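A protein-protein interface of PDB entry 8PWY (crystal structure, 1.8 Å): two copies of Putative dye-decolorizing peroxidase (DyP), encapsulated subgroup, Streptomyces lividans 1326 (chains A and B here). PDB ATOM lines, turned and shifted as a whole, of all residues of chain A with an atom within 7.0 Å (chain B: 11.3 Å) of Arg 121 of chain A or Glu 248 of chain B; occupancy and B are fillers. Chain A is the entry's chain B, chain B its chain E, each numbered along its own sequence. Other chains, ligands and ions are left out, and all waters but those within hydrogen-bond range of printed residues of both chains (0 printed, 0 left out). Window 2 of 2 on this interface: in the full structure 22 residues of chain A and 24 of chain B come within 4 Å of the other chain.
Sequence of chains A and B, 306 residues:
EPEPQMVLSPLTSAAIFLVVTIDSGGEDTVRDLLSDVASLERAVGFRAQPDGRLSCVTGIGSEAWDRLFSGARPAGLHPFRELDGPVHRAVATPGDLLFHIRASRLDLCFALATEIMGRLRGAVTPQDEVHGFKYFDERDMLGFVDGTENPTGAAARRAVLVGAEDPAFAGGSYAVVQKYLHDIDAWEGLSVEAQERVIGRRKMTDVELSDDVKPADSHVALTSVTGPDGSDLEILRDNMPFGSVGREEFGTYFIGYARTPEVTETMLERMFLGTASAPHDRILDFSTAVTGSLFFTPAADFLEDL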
ATOM      1  N   THR A  29     -28.849  -4.633  13.370  1.00  0.00           N
ATOM      2  CA  THR A  29     -27.411  -4.627  13.563  1.00  0.00           C
ATOM      3  C   THR A  29     -27.075  -4.203  14.999  1.00  0.00           C
ATOM      4  O   THR A  29     -26.224  -4.789  15.634  1.00  0.00           O
ATOM      5  CB  THR A  29     -26.735  -3.700  12.560  1.00  0.00           C
ATOM      6  OG1 THR A  29     -27.027  -4.223  11.281  1.00  0.00           O
ATOM      7  CG2 THR A  29     -25.236  -3.667  12.705  1.00  0.00           C
ATOM      8  N   ALA A 113     -13.344   0.418  21.406  1.00  0.00           N
ATOM      9  CA  ALA A 113     -14.169   1.301  20.601  1.00  0.00           C
ATOM     10  C   ALA A 113     -14.091   0.928  19.124  1.00  0.00           C
ATOM     11  O   ALA A 113     -15.089   0.973  18.424  1.00  0.00           O
ATOM     12  CB  ALA A 113     -13.783   2.760  20.779  1.00  0.00           C
ATOM     13  N   THR A 114     -12.905   0.570  18.658  1.00  0.00           N
ATOM     14  CA  THR A 114     -12.715   0.148  17.286  1.00  0.00           C
ATOM     15  C   THR A 114     -13.569  -1.085  16.985  1.00  0.00           C
ATOM     16  O   THR A 114     -14.214  -1.131  15.941  1.00  0.00           O
ATOM     17  CB  THR A 114     -11.230  -0.165  17.015  1.00  0.00           C
ATOM     18  OG1 THR A 114     -10.512   1.050  17.116  1.00  0.00           O
ATOM     19  CG2 THR A 114     -10.986  -0.690  15.628  1.00  0.00           C
ATOM     20  N   ILE A 116     -16.285  -2.159  18.549  1.00  0.00           N
ATOM     21  CA  ILE A 116     -17.692  -1.849  18.626  1.00  0.00           C
ATOM     22  C   ILE A 116     -18.141  -1.153  17.341  1.00  0.00           C
ATOM     23  O   ILE A 116     -19.114  -1.567  16.709  1.00  0.00           O
ATOM     24  CB  ILE A 116     -17.970  -1.057  19.905  1.00  0.00           C
ATOM     25  CG1 ILE A 116     -17.883  -1.995  21.115  1.00  0.00           C
ATOM     26  CG2 ILE A 116     -19.336  -0.370  19.809  1.00  0.00           C
ATOM     27  CD1 ILE A 116     -17.861  -1.292  22.405  1.00  0.00           C
ATOM     28  N   MET A 117     -17.422  -0.114  16.936  1.00  0.00           N
ATOM     29  CA  MET A 117     -17.841   0.671  15.790  1.00  0.00           C
ATOM     30  C   MET A 117     -17.700  -0.115  14.504  1.00  0.00           C
ATOM     31  O   MET A 117     -18.442   0.139  13.570  1.00  0.00           O
ATOM     32  CB  MET A 117     -17.022   1.953  15.669  1.00  0.00           C
ATOM     33  CG  MET A 117     -17.460   2.958  16.665  1.00  0.00           C
ATOM     34  SD  MET A 117     -19.104   3.627  16.353  1.00  0.00           S
ATOM     35  CE  MET A 117     -19.114   3.940  14.580  1.00  0.00           C
ATOM     36  N   GLY A 118     -16.737  -1.041  14.469  1.00  0.00           N
ATOM     37  CA  GLY A 118     -16.552  -1.967  13.372  1.00  0.00           C
ATOM     38  C   GLY A 118     -17.820  -2.763  13.097  1.00  0.00           C
ATOM     39  O   GLY A 118     -18.208  -2.946  11.952  1.00  0.00           O
ATOM     40  N   ARG A 119     -18.484  -3.200  14.154  1.00  0.00           N
ATOM     41  CA  ARG A 119     -19.700  -3.970  14.012  1.00  0.00           C
ATOM     42  C   ARG A 119     -20.890  -3.068  13.659  1.00  0.00           C
ATOM     43  O   ARG A 119     -21.902  -3.536  13.173  1.00  0.00           O
ATOM     44  CB  ARG A 119     -19.940  -4.726  15.320  1.00  0.00           C
ATOM     45  CG  ARG A 119     -18.819  -5.687  15.719  1.00  0.00           C
ATOM     46  CD  ARG A 119     -18.968  -7.112  15.184  1.00  0.00           C
ATOM     47  NE  ARG A 119     -20.354  -7.611  15.349  1.00  0.00           N
ATOM     48  CZ  ARG A 119     -20.768  -8.361  16.380  1.00  0.00           C
ATOM     49  NH1 ARG A 119     -19.845  -8.987  17.109  1.00  0.00           N
ATOM     50  NH2 ARG A 119     -22.067  -8.456  16.669  1.00  0.00           N
ATOM     51  N   LEU A 120     -20.817  -1.771  13.953  1.00  0.00           N
ATOM     52  CA  LEU A 120     -21.969  -0.902  13.785  1.00  0.00           C
ATOM     53  C   LEU A 120     -21.863  -0.073  12.505  1.00  0.00           C
ATOM     54  O   LEU A 120     -22.763   0.740  12.259  1.00  0.00           O
ATOM     55  CB  LEU A 120     -22.122   0.030  14.997  1.00  0.00           C
ATOM     56  CG  LEU A 120     -22.524  -0.657  16.297  1.00  0.00           C
ATOM     57  CD1 LEU A 120     -22.585   0.327  17.449  1.00  0.00           C
ATOM     58  CD2 LEU A 120     -23.856  -1.345  16.170  1.00  0.00           C
ATOM     59  N   ARG A 121     -20.761  -0.215  11.749  1.00  0.00           N
ATOM     60  CA  ARG A 121     -20.545   0.545  10.527  1.00  0.00           C
ATOM     61  C   ARG A 121     -21.812   0.436   9.659  1.00  0.00           C
ATOM     62  O   ARG A 121     -22.402  -0.629   9.464  1.00  0.00           O
ATOM     63  CB  ARG A 121     -19.414  -0.007   9.641  1.00  0.00           C
ATOM     64  CG  ARG A 121     -17.969   0.377   9.925  1.00  0.00           C
ATOM     65  CD  ARG A 121     -17.543   1.831  10.035  1.00  0.00           C
ATOM     66  NE  ARG A 121     -16.227   1.938  10.708  1.00  0.00           N
ATOM     67  CZ  ARG A 121     -15.915   2.758  11.735  1.00  0.00           C
ATOM     68  NH1 ARG A 121     -14.762   2.610  12.393  1.00  0.00           N
ATOM     69  NH2 ARG A 121     -16.746   3.724  12.119  1.00  0.00           N
ATOM     70  N   GLY A 122     -22.287   1.549   9.135  1.00  0.00           N
ATOM     71  CA  GLY A 122     -23.428   1.426   8.246  1.00  0.00           C
ATOM     72  C   GLY A 122     -24.751   1.415   8.981  1.00  0.00           C
ATOM     73  O   GLY A 122     -25.752   1.557   8.329  1.00  0.00           O
ATOM     74  N   ALA A 123     -24.805   1.257  10.300  1.00  0.00           N
ATOM     75  CA  ALA A 123     -26.080   1.261  11.001  1.00  0.00           C
ATOM     76  C   ALA A 123     -26.275   2.465  11.921  1.00  0.00           C
ATOM     77  O   ALA A 123     -27.398   2.690  12.398  1.00  0.00           O
ATOM     78  CB  ALA A 123     -26.178   0.007  11.820  1.00  0.00           C
ATOM     79  N   VAL A 124     -25.174   3.187  12.231  1.00  0.00           N
ATOM     80  CA  VAL A 124     -25.230   4.286  13.189  1.00  0.00           C
ATOM     81  C   VAL A 124     -24.492   5.477  12.597  1.00  0.00           C
ATOM     82  O   VAL A 124     -23.684   5.344  11.695  1.00  0.00           O
ATOM     83  CB  VAL A 124     -24.649   3.913  14.564  1.00  0.00           C
ATOM     84  CG1 VAL A 124     -25.331   2.711  15.171  1.00  0.00           C
ATOM     85  CG2 VAL A 124     -23.141   3.661  14.537  1.00  0.00           C
ATOM     86  N   PRO A 126     -22.111   8.649  14.139  1.00  0.00           N
ATOM     87  CA  PRO A 126     -21.503   9.240  15.328  1.00  0.00           C
ATOM     88  C   PRO A 126     -22.039  10.641  15.607  1.00  0.00           C
ATOM     89  O   PRO A 126     -22.145  11.421  14.707  1.00  0.00           O
ATOM     90  CB  PRO A 126     -20.007   9.314  15.005  1.00  0.00           C
ATOM     91  CG  PRO A 126     -19.825   8.484  13.768  1.00  0.00           C
ATOM     92  CD  PRO A 126     -21.159   8.440  13.049  1.00  0.00           C
ATOM     93  N   GLU A 129     -17.541  11.999  20.120  1.00  0.00           N
ATOM     94  CA  GLU A 129     -16.456  11.100  20.493  1.00  0.00           C
ATOM     95  C   GLU A 129     -15.464  11.914  21.302  1.00  0.00           C
ATOM     96  O   GLU A 129     -14.946  12.891  20.805  1.00  0.00           O
ATOM     97  CB  GLU A 129     -15.776  10.510  19.259  1.00  0.00           C
ATOM     98  CG  GLU A 129     -14.605   9.637  19.588  1.00  0.00           C
ATOM     99  CD  GLU A 129     -13.886   9.040  18.386  1.00  0.00           C
ATOM    100  OE1 GLU A 129     -14.267   9.380  17.252  1.00  0.00           O
ATOM    101  OE2 GLU A 129     -12.877   8.316  18.598  1.00  0.00           O
ATOM    102  N   PHE B 133      -0.829   7.240  21.307  1.00  0.00           N
ATOM    103  CA  PHE B 133      -0.901   6.263  22.381  1.00  0.00           C
ATOM    104  C   PHE B 133      -0.312   4.942  21.897  1.00  0.00           C
ATOM    105  O   PHE B 133      -0.627   4.468  20.833  1.00  0.00           O
ATOM    106  CB  PHE B 133      -2.347   6.053  22.821  1.00  0.00           C
ATOM    107  CG  PHE B 133      -3.362   5.865  21.706  1.00  0.00           C
ATOM    108  CD1 PHE B 133      -3.588   4.635  21.099  1.00  0.00           C
ATOM    109  CD2 PHE B 133      -4.096   6.954  21.251  1.00  0.00           C
ATOM    110  CE1 PHE B 133      -4.502   4.494  20.063  1.00  0.00           C
ATOM    111  CE2 PHE B 133      -5.050   6.798  20.248  1.00  0.00           C
ATOM    112  CZ  PHE B 133      -5.248   5.558  19.663  1.00  0.00           C
ATOM    113  N   MET B 141      -0.510   0.381  14.903  1.00  0.00           N
ATOM    114  CA  MET B 141      -1.869   0.256  14.408  1.00  0.00           C
ATOM    115  C   MET B 141      -2.012  -0.922  13.439  1.00  0.00           C
ATOM    116  O   MET B 141      -3.087  -1.392  13.194  1.00  0.00           O
ATOM    117  CB  MET B 141      -2.199   1.598  13.751  1.00  0.00           C
ATOM    118  CG  MET B 141      -3.653   1.914  13.470  1.00  0.00           C
ATOM    119  SD  MET B 141      -4.579   1.869  14.942  1.00  0.00           S
ATOM    120  CE  MET B 141      -4.572   3.558  15.543  1.00  0.00           C
ATOM    121  N   TYR B 180       0.968   9.407   8.834  1.00  0.00           N
ATOM    122  CA  TYR B 180       0.431   8.390   7.927  1.00  0.00           C
ATOM    123  C   TYR B 180      -0.982   7.995   8.365  1.00  0.00           C
ATOM    124  O   TYR B 180      -1.235   7.802   9.553  1.00  0.00           O
ATOM    125  CB  TYR B 180       1.290   7.142   7.888  1.00  0.00           C
ATOM    126  CG  TYR B 180       2.600   7.246   7.125  1.00  0.00           C
ATOM    127  CD1 TYR B 180       2.666   6.965   5.760  1.00  0.00           C
ATOM    128  CD2 TYR B 180       3.776   7.645   7.754  1.00  0.00           C
ATOM    129  CE1 TYR B 180       3.864   7.096   5.067  1.00  0.00           C
ATOM    130  CE2 TYR B 180       4.977   7.782   7.076  1.00  0.00           C
ATOM    131  CZ  TYR B 180       5.035   7.484   5.727  1.00  0.00           C
ATOM    132  OH  TYR B 180       6.252   7.580   5.133  1.00  0.00           O
ATOM    133  N   LEU B 181      -1.895   7.850   7.406  1.00  0.00           N
ATOM    134  CA  LEU B 181      -3.188   7.224   7.649  1.00  0.00           C
ATOM    135  C   LEU B 181      -3.207   5.863   6.962  1.00  0.00           C
ATOM    136  O   LEU B 181      -2.680   5.721   5.854  1.00  0.00           O
ATOM    137  CB  LEU B 181      -4.303   8.102   7.085  1.00  0.00           C
ATOM    138  CG  LEU B 181      -4.400   9.496   7.701  1.00  0.00           C
ATOM    139  CD1 LEU B 181      -5.327  10.374   6.883  1.00  0.00           C
ATOM    140  CD2 LEU B 181      -4.842   9.420   9.154  1.00  0.00           C
ATOM    141  N   HIS B 182      -3.830   4.881   7.601  1.00  0.00           N
ATOM    142  CA  HIS B 182      -3.787   3.526   7.105  1.00  0.00           C
ATOM    143  C   HIS B 182      -5.154   3.152   6.556  1.00  0.00           C
ATOM    144  O   HIS B 182      -6.199   3.626   7.039  1.00  0.00           O
ATOM    145  CB  HIS B 182      -3.429   2.542   8.214  1.00  0.00           C
ATOM    146  CG  HIS B 182      -2.058   2.713   8.736  1.00  0.00           C
ATOM    147  ND1 HIS B 182      -0.934   2.455   7.986  1.00  0.00           N
ATOM    148  CD2 HIS B 182      -1.644   3.072   9.945  1.00  0.00           C
ATOM    149  CE1 HIS B 182       0.135   2.673   8.730  1.00  0.00           C
ATOM    150  NE2 HIS B 182      -0.262   3.054   9.943  1.00  0.00           N
ATOM    151  N   ASP B 183      -5.126   2.245   5.575  1.00  0.00           N
ATOM    152  CA  ASP B 183      -6.326   1.566   5.124  1.00  0.00           C
ATOM    153  C   ASP B 183      -6.411   0.246   5.881  1.00  0.00           C
ATOM    154  O   ASP B 183      -5.888  -0.792   5.445  1.00  0.00           O
ATOM    155  CB  ASP B 183      -6.262   1.436   3.602  1.00  0.00           C
ATOM    156  CG  ASP B 183      -7.484   0.812   2.989  1.00  0.00           C
ATOM    157  OD1 ASP B 183      -8.368   0.321   3.728  1.00  0.00           O
ATOM    158  OD2 ASP B 183      -7.505   0.812   1.774  1.00  0.00           O
ATOM    159  N   ILE B 184      -7.069   0.295   7.033  1.00  0.00           N
ATOM    160  CA  ILE B 184      -7.161  -0.858   7.914  1.00  0.00           C
ATOM    161  C   ILE B 184      -7.981  -1.992   7.288  1.00  0.00           C
ATOM    162  O   ILE B 184      -7.644  -3.164   7.459  1.00  0.00           O
ATOM    163  CB  ILE B 184      -7.700  -0.414   9.287  1.00  0.00           C
ATOM    164  CG1 ILE B 184      -6.669   0.440  10.017  1.00  0.00           C
ATOM    165  CG2 ILE B 184      -8.005  -1.615  10.140  1.00  0.00           C
ATOM    166  CD1 ILE B 184      -5.370  -0.277  10.365  1.00  0.00           C
ATOM    167  N   ASP B 185      -9.023  -1.670   6.530  1.00  0.00           N
ATOM    168  CA  ASP B 185      -9.856  -2.696   5.908  1.00  0.00           C
ATOM    169  C   ASP B 185      -9.019  -3.496   4.932  1.00  0.00           C
ATOM    170  O   ASP B 185      -9.085  -4.694   4.921  1.00  0.00           O
ATOM    171  CB  ASP B 185     -11.030  -2.096   5.129  1.00  0.00           C
ATOM    172  CG  ASP B 185     -12.067  -1.423   6.003  1.00  0.00           C
ATOM    173  OD1 ASP B 185     -12.182  -1.775   7.191  1.00  0.00           O
ATOM    174  OD2 ASP B 185     -12.730  -0.526   5.492  1.00  0.00           O
ATOM    175  N   ALA B 186      -8.218  -2.839   4.115  1.00  0.00           N
ATOM    176  CA  ALA B 186      -7.367  -3.567   3.200  1.00  0.00           C
ATOM    177  C   ALA B 186      -6.357  -4.430   3.944  1.00  0.00           C
ATOM    178  O   ALA B 186      -6.115  -5.574   3.560  1.00  0.00           O
ATOM    179  CB  ALA B 186      -6.660  -2.595   2.270  1.00  0.00           C
ATOM    180  N   GLU B 188      -6.412  -5.694   6.965  1.00  0.00           N
ATOM    181  CA  GLU B 188      -7.031  -6.810   7.665  1.00  0.00           C
ATOM    182  C   GLU B 188      -7.579  -7.846   6.706  1.00  0.00           C
ATOM    183  O   GLU B 188      -7.880  -8.938   7.105  1.00  0.00           O
ATOM    184  CB  GLU B 188      -8.006  -6.295   8.730  1.00  0.00           C
ATOM    185  CG  GLU B 188      -7.178  -6.062   9.997  1.00  0.00           C
ATOM    186  CD  GLU B 188      -7.786  -5.228  11.092  1.00  0.00           C
ATOM    187  OE1 GLU B 188      -8.986  -4.916  10.983  1.00  0.00           O
ATOM    188  OE2 GLU B 188      -7.018  -4.802  11.974  1.00  0.00           O
ATOM    189  N   PHE B 242      -2.391   6.789  16.406  1.00  0.00           N
ATOM    190  CA  PHE B 242      -3.378   7.781  16.779  1.00  0.00           C
ATOM    191  C   PHE B 242      -4.622   7.469  15.970  1.00  0.00           C
ATOM    192  O   PHE B 242      -4.565   6.727  15.013  1.00  0.00           O
ATOM    193  CB  PHE B 242      -2.900   9.210  16.478  1.00  0.00           C
ATOM    194  CG  PHE B 242      -2.779   9.505  15.000  1.00  0.00           C
ATOM    195  CD1 PHE B 242      -1.631   9.164  14.286  1.00  0.00           C
ATOM    196  CD2 PHE B 242      -3.826  10.080  14.314  1.00  0.00           C
ATOM    197  CE1 PHE B 242      -1.531   9.445  12.940  1.00  0.00           C
ATOM    198  CE2 PHE B 242      -3.727  10.359  12.960  1.00  0.00           C
ATOM    199  CZ  PHE B 242      -2.590  10.015  12.281  1.00  0.00           C
ATOM    200  N   GLY B 243      -5.729   8.052  16.394  1.00  0.00           N
ATOM    201  CA  GLY B 243      -6.884   7.970  15.572  1.00  0.00           C
ATOM    202  C   GLY B 243      -8.160   8.521  16.199  1.00  0.00           C
ATOM    203  O   GLY B 243      -8.212   9.016  17.318  1.00  0.00           O
ATOM    204  N   SER B 244      -9.223   8.277  15.444  1.00  0.00           N
ATOM    205  CA  SER B 244     -10.579   8.626  15.811  1.00  0.00           C
ATOM    206  C   SER B 244     -11.523   7.571  15.229  1.00  0.00           C
ATOM    207  O   SER B 244     -11.537   7.356  14.015  1.00  0.00           O
ATOM    208  CB  SER B 244     -10.847  10.020  15.321  1.00  0.00           C
ATOM    209  OG  SER B 244     -12.233  10.220  15.195  1.00  0.00           O
ATOM    210  N   VAL B 245     -12.279   6.863  16.080  1.00  0.00           N
ATOM    211  CA  VAL B 245     -13.090   5.766  15.551  1.00  0.00           C
ATOM    212  C   VAL B 245     -14.292   6.314  14.788  1.00  0.00           C
ATOM    213  O   VAL B 245     -14.695   5.742  13.807  1.00  0.00           O
ATOM    214  CB  VAL B 245     -13.517   4.731  16.607  1.00  0.00           C
ATOM    215  CG1 VAL B 245     -12.312   4.011  17.152  1.00  0.00           C
ATOM    216  CG2 VAL B 245     -14.331   5.339  17.727  1.00  0.00           C
ATOM    217  N   GLY B 246     -14.830   7.444  15.208  1.00  0.00           N
ATOM    218  CA  GLY B 246     -15.998   8.013  14.571  1.00  0.00           C
ATOM    219  C   GLY B 246     -15.714   8.459  13.137  1.00  0.00           C
ATOM    220  O   GLY B 246     -16.538   8.297  12.243  1.00  0.00           O
ATOM    221  N   ARG B 247     -14.538   9.037  12.926  1.00  0.00           N
ATOM    222  CA  ARG B 247     -14.113   9.493  11.620  1.00  0.00           C
ATOM    223  C   ARG B 247     -13.392   8.388  10.847  1.00  0.00           C
ATOM    224  O   ARG B 247     -12.909   8.635   9.781  1.00  0.00           O
ATOM    225  CB  ARG B 247     -13.187  10.697  11.795  1.00  0.00           C
ATOM    226  CG  ARG B 247     -13.905  11.973  12.226  1.00  0.00           C
ATOM    227  CD  ARG B 247     -13.270  13.266  11.723  1.00  0.00           C
ATOM    228  NE  ARG B 247     -11.846  13.267  12.043  1.00  0.00           N
ATOM    229  CZ  ARG B 247     -11.330  13.258  13.281  1.00  0.00           C
ATOM    230  NH1 ARG B 247     -12.092  13.475  14.344  1.00  0.00           N
ATOM    231  NH2 ARG B 247     -10.032  13.057  13.444  1.00  0.00           N
ATOM    232  N   GLU B 248     -13.299   7.164  11.350  1.00  0.00           N
ATOM    233  CA  GLU B 248     -12.562   6.109  10.676  1.00  0.00           C
ATOM    234  C   GLU B 248     -11.118   6.492  10.340  1.00  0.00           C
ATOM    235  O   GLU B 248     -10.630   6.137   9.283  1.00  0.00           O
ATOM    236  CB  GLU B 248     -13.246   5.731   9.370  1.00  0.00           C
ATOM    237  CG  GLU B 248     -14.447   4.863   9.577  1.00  0.00           C
ATOM    238  CD  GLU B 248     -15.199   4.525   8.292  1.00  0.00           C
ATOM    239  OE1 GLU B 248     -14.610   3.896   7.378  1.00  0.00           O
ATOM    240  OE2 GLU B 248     -16.388   4.899   8.193  1.00  0.00           O
ATOM    241  N   GLU B 249     -10.410   7.163  11.239  1.00  0.00           N
ATOM    242  CA  GLU B 249      -9.025   7.532  11.039  1.00  0.00           C
ATOM    243  C   GLU B 249      -8.153   6.648  11.917  1.00  0.00           C
ATOM    244  O   GLU B 249      -8.277   6.682  13.156  1.00  0.00           O
ATOM    245  CB  GLU B 249      -8.770   8.968  11.471  1.00  0.00           C
ATOM    246  CG  GLU B 249      -9.037   9.949  10.369  1.00  0.00           C
ATOM    247  CD  GLU B 249      -8.738  11.375  10.794  1.00  0.00           C
ATOM    248  OE1 GLU B 249      -9.480  12.239  10.317  1.00  0.00           O
ATOM    249  OE2 GLU B 249      -7.758  11.605  11.626  1.00  0.00           O
ATOM    250  N   PHE B 250      -7.292   5.857  11.273  1.00  0.00           N
ATOM    251  CA  PHE B 250      -6.364   5.015  12.001  1.00  0.00           C
ATOM    252  C   PHE B 250      -4.969   5.288  11.465  1.00  0.00           C
ATOM    253  O   PHE B 250      -4.733   5.136  10.300  1.00  0.00           O
ATOM    254  CB  PHE B 250      -6.729   3.544  11.860  1.00  0.00           C
ATOM    255  CG  PHE B 250      -8.161   3.262  12.198  1.00  0.00           C
ATOM    256  CD1 PHE B 250      -8.508   3.075  13.521  1.00  0.00           C
ATOM    257  CD2 PHE B 250      -9.147   3.190  11.227  1.00  0.00           C
ATOM    258  CE1 PHE B 250      -9.826   2.830  13.880  1.00  0.00           C
ATOM    259  CE2 PHE B 250     -10.463   2.963  11.594  1.00  0.00           C
ATOM    260  CZ  PHE B 250     -10.805   2.823  12.923  1.00  0.00           C
ATOM    261  N   GLY B 251      -4.045   5.724  12.301  1.00  0.00           N
ATOM    262  CA  GLY B 251      -2.847   6.376  11.814  1.00  0.00           C
ATOM    263  C   GLY B 251      -1.595   5.939  12.560  1.00  0.00           C
ATOM    264  O   GLY B 251      -1.671   5.320  13.603  1.00  0.00           O
ATOM    265  N   THR B 252      -0.453   6.193  11.932  1.00  0.00           N
ATOM    266  CA  THR B 252       0.845   6.099  12.530  1.00  0.00           C
ATOM    267  C   THR B 252       1.514   7.450  12.366  1.00  0.00           C
ATOM    268  O   THR B 252       1.644   7.926  11.249  1.00  0.00           O
ATOM    269  CB  THR B 252       1.709   5.016  11.882  1.00  0.00           C
ATOM    270  OG1 THR B 252       1.108   3.734  12.075  1.00  0.00           O
ATOM    271  CG2 THR B 252       3.102   4.992  12.484  1.00  0.00           C
ATOM    272  N   PHE B 286      -0.621   0.398   2.112  1.00  0.00           N
ATOM    273  CA  PHE B 286      -1.614   0.452   3.174  1.00  0.00           C
ATOM    274  C   PHE B 286      -1.479   1.714   4.013  1.00  0.00           C
ATOM    275  O   PHE B 286      -2.117   1.826   5.054  1.00  0.00           O
ATOM    276  CB  PHE B 286      -1.416  -0.771   4.082  1.00  0.00           C
ATOM    277  CG  PHE B 286      -1.509  -2.050   3.297  1.00  0.00           C
ATOM    278  CD1 PHE B 286      -2.758  -2.561   2.939  1.00  0.00           C
ATOM    279  CD2 PHE B 286      -0.368  -2.647   2.781  1.00  0.00           C
ATOM    280  CE1 PHE B 286      -2.853  -3.705   2.175  1.00  0.00           C
ATOM    281  CE2 PHE B 286      -0.475  -3.793   2.020  1.00  0.00           C
ATOM    282  CZ  PHE B 286      -1.707  -4.301   1.708  1.00  0.00           C
ATOM    283  N   THR B 288      -0.810   6.109   3.752  1.00  0.00           N
ATOM    284  CA  THR B 288      -0.676   7.339   2.984  1.00  0.00           C
ATOM    285  C   THR B 288      -0.107   8.463   3.852  1.00  0.00           C
ATOM    286  O   THR B 288      -0.717   8.767   4.890  1.00  0.00           O
ATOM    287  CB  THR B 288      -2.045   7.779   2.475  1.00  0.00           C
ATOM    288  OG1 THR B 288      -2.475   6.674   1.701  1.00  0.00           O
ATOM    289  CG2 THR B 288      -2.043   9.038   1.649  1.00  0.00           C
ATOM    290  N   VAL B 290       0.317  12.222   4.799  1.00  0.00           N
ATOM    291  CA  VAL B 290      -0.452  13.445   4.603  1.00  0.00           C
ATOM    292  C   VAL B 290       0.270  14.668   5.180  1.00  0.00           C
ATOM    293  O   VAL B 290      -0.201  15.783   4.980  1.00  0.00           O
ATOM    294  CB  VAL B 290      -1.884  13.337   5.160  1.00  0.00           C
ATOM    295  CG1 VAL B 290      -2.580  12.130   4.577  1.00  0.00           C
ATOM    296  CG2 VAL B 290      -1.902  13.224   6.661  1.00  0.00           C
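The side-chain carboxylate (OE1) of Glu 129 of chain A lies within hydrogen-bond range of the backbone NH (N) of Gly 246 of chain B, at 2.9 Å. The guanidinium group (NE) of Arg 121 of chain A is in salt-bridge range of the side-chain carboxylate (OE2) of Glu 248 of chain B, at 3.9 Å. The guanidinium group of Arg 121 of chain A lies within hydrogen-bond range of the backbone carbonyl oxygen of Val 245 of chain B (3.3 Å). The side-chain carboxylate (OE2) of Glu 129 of chain A lies within hydrogen-bond range of the backbone NH (N) of Val 245 of chain B, at 3.0 Å. The side-chain carboxylate of Glu 129 of chain A sits at hydrogen-bond distance from the side-chain hydroxyl of Ser 244 of chain B, at 3.0 Å.
The side-chain hydroxyl (OG) of Ser 244 of chain B sits at hydrogen-bond distance from the guanidinium group (NH1) of Arg 247 of chain B (3.4 Å). The backbone carbonyl oxygen of Phe 250 of chain B sits at hydrogen-bond distance from the backbone NH of His 182 of chain B (2.9 Å). The backbone NH of Ser 244 of chain B lies within hydrogen-bond range of the backbone carbonyl oxygen of Glu 249 of chain B (2.9 Å).
Thr 114 of chain A touches Val 245 of chain B (OG1 to CG1, 3.5 Å). Thr 114 of chain A touches Phe 250 of chain B. Arg 121 of chain A touches Phe 250 of chain B (NH1 to CZ, 3.998 Å). CG of Pro 126 of chain A touches O of Gly 246 of chain B, at 3.6 Å.
No residue of chain B comes within 4 Å of Met 117 of chain A. No residue of chain B comes within 4 Å of Gly 118 of chain A. Leu 120 of chain A touches none of the printed residues of chain B. Of the printed residues of chain B, Arg 121 of chain A touches Val 245 (3.3 Å), Glu 248 (3.4 Å) and Phe 250 (3.998 Å). No residue of chain B comes within 4 Å of Ala 123 of chain A. No residue of chain B comes within 4 Å of Val 124 of chain A. Of the printed residues of chain B, Pro 126 of chain A touches Gly 246. Of the printed residues of chain B, Glu 129 of chain A touches Ser 244 (3.0 Å), Val 245 (3.0 Å) and Gly 246 (2.9 Å). Of the printed residues of chain A, Ser 244 of chain B touches Glu 129. Printed residues of chain A within 4 Å of Val 245 of chain B: Thr 114, Arg 121 and Glu 129. Of the printed residues of chain A, Gly 246 of chain B touches Pro 126 (3.6 Å) and Glu 129 (2.9 Å). Glu 248 of chain B touches just one residue of chain A: Arg 121 (3.4 Å). The nearest residue of chain A that does not touch Glu 248 of chain B is Glu 129 of chain A (6.4 Å). The nearest printed residue of chain B that does not touch Pro 126 of chain A is Arg 247 of chain B (5.4 Å).
Of the 14 printed residues of chain A, 4 touch a printed residue of chain B. Hydrophobic or aromatic side chains of chain A that line the printed part of chain B: Pro 126. Along chain A the printed residues that touch a printed residue of chain B span positions 114 to 129. Of the 24 printed residues of chain B, 5 touch a printed residue of chain A. Printed residues of chain B that touch a printed residue of chain A: Ser 244, Val 245, Gly 246, Glu 248 and Phe 250. Among the printed residues, Asp or Glu carboxylates within 4 Å of a Lys or Arg side-chain nitrogen of the other chain: Arg 121 of chain A with Glu 248 of chain B (3.9 Å).
No position is printed for both chains.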
